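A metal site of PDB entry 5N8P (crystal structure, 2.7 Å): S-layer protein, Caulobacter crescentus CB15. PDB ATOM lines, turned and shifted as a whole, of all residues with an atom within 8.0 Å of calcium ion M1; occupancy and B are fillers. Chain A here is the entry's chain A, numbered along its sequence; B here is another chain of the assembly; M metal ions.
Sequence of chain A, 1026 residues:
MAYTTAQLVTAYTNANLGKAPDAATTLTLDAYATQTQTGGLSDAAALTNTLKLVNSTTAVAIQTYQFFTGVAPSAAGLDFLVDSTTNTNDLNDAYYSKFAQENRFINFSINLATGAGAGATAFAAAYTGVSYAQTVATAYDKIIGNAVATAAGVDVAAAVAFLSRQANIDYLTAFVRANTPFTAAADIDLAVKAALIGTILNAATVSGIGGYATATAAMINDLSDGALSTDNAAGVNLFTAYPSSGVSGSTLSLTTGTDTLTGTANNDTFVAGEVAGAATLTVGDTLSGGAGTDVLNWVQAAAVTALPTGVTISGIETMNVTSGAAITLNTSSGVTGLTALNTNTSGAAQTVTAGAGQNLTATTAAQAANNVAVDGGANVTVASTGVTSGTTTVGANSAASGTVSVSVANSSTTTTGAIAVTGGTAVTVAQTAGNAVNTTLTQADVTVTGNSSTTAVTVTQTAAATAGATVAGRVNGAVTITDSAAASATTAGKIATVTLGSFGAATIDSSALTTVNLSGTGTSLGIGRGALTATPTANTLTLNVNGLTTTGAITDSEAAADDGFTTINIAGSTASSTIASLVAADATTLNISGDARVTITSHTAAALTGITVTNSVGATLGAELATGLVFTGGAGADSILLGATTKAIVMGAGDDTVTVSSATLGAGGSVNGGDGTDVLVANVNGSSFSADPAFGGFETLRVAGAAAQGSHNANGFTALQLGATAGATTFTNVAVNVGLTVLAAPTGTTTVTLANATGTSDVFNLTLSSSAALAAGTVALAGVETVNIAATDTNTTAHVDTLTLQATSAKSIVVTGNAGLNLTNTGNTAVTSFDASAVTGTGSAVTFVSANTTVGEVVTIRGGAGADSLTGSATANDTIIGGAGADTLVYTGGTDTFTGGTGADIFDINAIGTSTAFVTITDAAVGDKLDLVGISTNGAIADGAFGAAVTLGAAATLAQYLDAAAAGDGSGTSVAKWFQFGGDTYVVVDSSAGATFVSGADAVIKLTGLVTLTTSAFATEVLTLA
The backbone NH (N) of Gly 783 sits close to the side-chain hydroxyl (OG) of Ser 809, 3.5 Å away. OE2 of Glu 785 lies within hydrogen-bond range of N of Ser 761 (3.3 Å). N of Thr 786 is in hydrogen-bond range of O of Asp 762 (2.9 Å).
Five residues have an atom within 4 Å of calcium ion M1: Ala 757, Gly 759, Asp 762, Gly 783 and Glu 785. Along chain A the residues within 4 Å of calcium ion M1 span positions 757 to 785.
The backbone carbonyl oxygen (O) of Gly 783 is bound to calcium ion M1 (2.4 Å). Calcium ion M1 is bound by O of Ala 757 (2.4 Å). OE1 of Glu 785 is bound to calcium ion M1, at 2.5 Å. Calcium ion M1 is bound by OD2 of Asp 762 (2.6 Å). O of Gly 759 binds calcium ion M1. Calcium ion M1 has five donor atoms within binding distance. Slightly farther from calcium ion M1 lies the side-chain carboxylate (OE2) of Glu 785 (3.0 Å).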
ATOM      1  N   LEU A 754      31.053  22.754   1.602  1.00  0.00           N
ATOM      2  CA  LEU A 754      30.786  21.897   0.448  1.00  0.00           C
ATOM      3  C   LEU A 754      32.036  21.622  -0.340  1.00  0.00           C
ATOM      4  O   LEU A 754      33.045  22.347  -0.245  1.00  0.00           O
ATOM      5  CB  LEU A 754      29.710  22.475  -0.476  1.00  0.00           C
ATOM      6  CG  LEU A 754      28.278  22.676   0.030  1.00  0.00           C
ATOM      7  CD1 LEU A 754      28.223  24.008   0.741  1.00  0.00           C
ATOM      8  CD2 LEU A 754      27.255  22.636  -1.094  1.00  0.00           C
ATOM      9  N   ASN A 756      32.137  21.945  -3.606  1.00  0.00           N
ATOM     10  CA  ASN A 756      32.200  23.125  -4.449  1.00  0.00           C
ATOM     11  C   ASN A 756      31.086  24.156  -4.208  1.00  0.00           C
ATOM     12  O   ASN A 756      29.956  23.966  -4.669  1.00  0.00           O
ATOM     13  CB  ASN A 756      32.212  22.676  -5.897  1.00  0.00           C
ATOM     14  CG  ASN A 756      32.410  23.832  -6.880  1.00  0.00           C
ATOM     15  OD1 ASN A 756      32.964  24.867  -6.526  1.00  0.00           O
ATOM     16  ND2 ASN A 756      31.943  23.655  -8.096  1.00  0.00           N
ATOM     17  N   ALA A 757      31.414  25.255  -3.551  1.00  0.00           N
ATOM     18  CA  ALA A 757      30.408  26.286  -3.264  1.00  0.00           C
ATOM     19  C   ALA A 757      30.264  27.348  -4.369  1.00  0.00           C
ATOM     20  O   ALA A 757      29.386  28.199  -4.296  1.00  0.00           O
ATOM     21  CB  ALA A 757      30.698  26.948  -1.916  1.00  0.00           C
ATOM     22  N   THR A 758      31.111  27.283  -5.394  1.00  0.00           N
ATOM     23  CA  THR A 758      31.379  28.448  -6.266  1.00  0.00           C
ATOM     24  C   THR A 758      30.231  28.909  -7.169  1.00  0.00           C
ATOM     25  O   THR A 758      30.129  30.109  -7.423  1.00  0.00           O
ATOM     26  CB  THR A 758      32.632  28.259  -7.129  1.00  0.00           C
ATOM     27  OG1 THR A 758      32.422  27.200  -8.041  1.00  0.00           O
ATOM     28  CG2 THR A 758      33.869  27.970  -6.286  1.00  0.00           C
ATOM     29  N   GLY A 759      29.395  27.968  -7.650  1.00  0.00           N
ATOM     30  CA  GLY A 759      28.168  28.245  -8.445  1.00  0.00           C
ATOM     31  C   GLY A 759      27.153  29.170  -7.772  1.00  0.00           C
ATOM     32  O   GLY A 759      27.364  29.629  -6.660  1.00  0.00           O
ATOM     33  N   THR A 760      26.056  29.480  -8.447  1.00  0.00           N
ATOM     34  CA  THR A 760      25.078  30.457  -7.892  1.00  0.00           C
ATOM     35  C   THR A 760      23.682  29.843  -7.661  1.00  0.00           C
ATOM     36  O   THR A 760      22.709  30.562  -7.419  1.00  0.00           O
ATOM     37  CB  THR A 760      24.987  31.733  -8.770  1.00  0.00           C
ATOM     38  OG1 THR A 760      24.928  31.356 -10.162  1.00  0.00           O
ATOM     39  CG2 THR A 760      26.182  32.697  -8.520  1.00  0.00           C
ATOM     40  N   SER A 761      23.610  28.508  -7.741  1.00  0.00           N
ATOM     41  CA  SER A 761      22.388  27.717  -7.596  1.00  0.00           C
ATOM     42  C   SER A 761      22.616  26.621  -6.572  1.00  0.00           C
ATOM     43  O   SER A 761      22.125  25.490  -6.750  1.00  0.00           O
ATOM     44  CB  SER A 761      22.062  27.034  -8.924  1.00  0.00           C
ATOM     45  OG  SER A 761      21.817  27.961  -9.950  1.00  0.00           O
ATOM     46  N   ASP A 762      23.358  26.942  -5.510  1.00  0.00           N
ATOM     47  CA  ASP A 762      23.709  25.938  -4.511  1.00  0.00           C
ATOM     48  C   ASP A 762      22.561  25.650  -3.546  1.00  0.00           C
ATOM     49  O   ASP A 762      22.004  26.573  -2.949  1.00  0.00           O
ATOM     50  CB  ASP A 762      25.032  26.293  -3.821  1.00  0.00           C
ATOM     51  CG  ASP A 762      26.185  26.413  -4.813  1.00  0.00           C
ATOM     52  OD1 ASP A 762      26.556  25.400  -5.427  1.00  0.00           O
ATOM     53  OD2 ASP A 762      26.705  27.516  -4.986  1.00  0.00           O
ATOM     54  N   VAL A 763      22.193  24.369  -3.434  1.00  0.00           N
ATOM     55  CA  VAL A 763      21.062  23.896  -2.613  1.00  0.00           C
ATOM     56  C   VAL A 763      21.580  23.000  -1.491  1.00  0.00           C
ATOM     57  O   VAL A 763      22.326  22.043  -1.732  1.00  0.00           O
ATOM     58  CB  VAL A 763      20.043  23.095  -3.445  1.00  0.00           C
ATOM     59  CG1 VAL A 763      18.759  22.875  -2.669  1.00  0.00           C
ATOM     60  CG2 VAL A 763      19.725  23.767  -4.765  1.00  0.00           C
ATOM     61  N   LEU A 781      26.468  27.619   6.755  1.00  0.00           N
ATOM     62  CA  LEU A 781      26.454  27.101   5.377  1.00  0.00           C
ATOM     63  C   LEU A 781      26.918  28.145   4.362  1.00  0.00           C
ATOM     64  O   LEU A 781      26.140  28.545   3.461  1.00  0.00           O
ATOM     65  CB  LEU A 781      25.057  26.610   5.003  1.00  0.00           C
ATOM     66  CG  LEU A 781      24.497  25.383   5.690  1.00  0.00           C
ATOM     67  CD1 LEU A 781      22.994  25.387   5.506  1.00  0.00           C
ATOM     68  CD2 LEU A 781      25.043  24.171   4.993  1.00  0.00           C
ATOM     69  N   ALA A 782      28.180  28.601   4.509  1.00  0.00           N
ATOM     70  CA  ALA A 782      28.825  29.543   3.565  1.00  0.00           C
ATOM     71  C   ALA A 782      28.644  29.070   2.103  1.00  0.00           C
ATOM     72  O   ALA A 782      28.747  27.850   1.816  1.00  0.00           O
ATOM     73  CB  ALA A 782      30.303  29.681   3.905  1.00  0.00           C
ATOM     74  N   GLY A 783      28.316  30.017   1.210  1.00  0.00           N
ATOM     75  CA  GLY A 783      28.163  29.767  -0.232  1.00  0.00           C
ATOM     76  C   GLY A 783      26.958  28.995  -0.792  1.00  0.00           C
ATOM     77  O   GLY A 783      26.920  28.638  -1.988  1.00  0.00           O
ATOM     78  N   VAL A 784      25.955  28.751   0.053  1.00  0.00           N
ATOM     79  CA  VAL A 784      24.715  28.093  -0.351  1.00  0.00           C
ATOM     80  C   VAL A 784      23.623  29.120  -0.603  1.00  0.00           C
ATOM     81  O   VAL A 784      23.427  30.034   0.193  1.00  0.00           O
ATOM     82  CB  VAL A 784      24.277  27.062   0.724  1.00  0.00           C
ATOM     83  CG1 VAL A 784      23.136  26.162   0.241  1.00  0.00           C
ATOM     84  CG2 VAL A 784      25.477  26.247   1.178  1.00  0.00           C
ATOM     85  N   GLU A 785      22.896  28.968  -1.717  1.00  0.00           N
ATOM     86  CA  GLU A 785      21.926  29.987  -2.188  1.00  0.00           C
ATOM     87  C   GLU A 785      20.480  29.723  -1.798  1.00  0.00           C
ATOM     88  O   GLU A 785      19.723  30.657  -1.533  1.00  0.00           O
ATOM     89  CB  GLU A 785      22.037  30.145  -3.707  1.00  0.00           C
ATOM     90  CG  GLU A 785      23.157  31.073  -4.169  1.00  0.00           C
ATOM     91  CD  GLU A 785      24.543  30.426  -4.222  1.00  0.00           C
ATOM     92  OE1 GLU A 785      25.517  31.115  -3.830  1.00  0.00           O
ATOM     93  OE2 GLU A 785      24.668  29.243  -4.661  1.00  0.00           O
ATOM     94  N   THR A 786      20.113  28.437  -1.834  1.00  0.00           N
ATOM     95  CA  THR A 786      18.847  27.933  -1.341  1.00  0.00           C
ATOM     96  C   THR A 786      19.139  26.993  -0.158  1.00  0.00           C
ATOM     97  O   THR A 786      19.848  25.992  -0.304  1.00  0.00           O
ATOM     98  CB  THR A 786      18.084  27.186  -2.464  1.00  0.00           C
ATOM     99  OG1 THR A 786      17.829  28.085  -3.560  1.00  0.00           O
ATOM    100  CG2 THR A 786      16.749  26.591  -1.946  1.00  0.00           C
ATOM    101  N   SER A 809      25.075  33.875   1.906  1.00  0.00           N
ATOM    102  CA  SER A 809      24.717  34.026   0.489  1.00  0.00           C
ATOM    103  C   SER A 809      23.428  33.265   0.083  1.00  0.00           C
ATOM    104  O   SER A 809      23.203  32.921  -1.091  1.00  0.00           O
ATOM    105  CB  SER A 809      25.886  33.749  -0.482  1.00  0.00           C
ATOM    106  OG  SER A 809      26.885  32.959   0.087  1.00  0.00           O
ATOM    107  N   ALA A 810      22.590  33.012   1.081  1.00  0.00           N
ATOM    108  CA  ALA A 810      21.339  32.394   0.773  1.00  0.00           C
ATOM    109  C   ALA A 810      20.353  33.491   0.384  1.00  0.00           C
ATOM    110  O   ALA A 810      20.250  34.515   1.085  1.00  0.00           O
ATOM    111  CB  ALA A 810      20.860  31.564   1.934  1.00  0.00           C
ATOM    112  N   ALA B 667      33.420  31.873 -10.070  1.00  0.00           N
ATOM    113  CA  ALA B 667      32.280  31.923 -11.021  1.00  0.00           C
ATOM    114  C   ALA B 667      31.917  30.504 -11.406  1.00  0.00           C
ATOM    115  O   ALA B 667      31.287  29.829 -10.624  1.00  0.00           O
ATOM    116  CB  ALA B 667      32.589  32.792 -12.274  1.00  0.00           C
HETATM  117 CA    CA M   1      27.590  29.714  -3.975  1.00  0.00          CA
HETATM  118 CA    CA M   2      25.358  30.944   2.115  1.00  0.00          CA
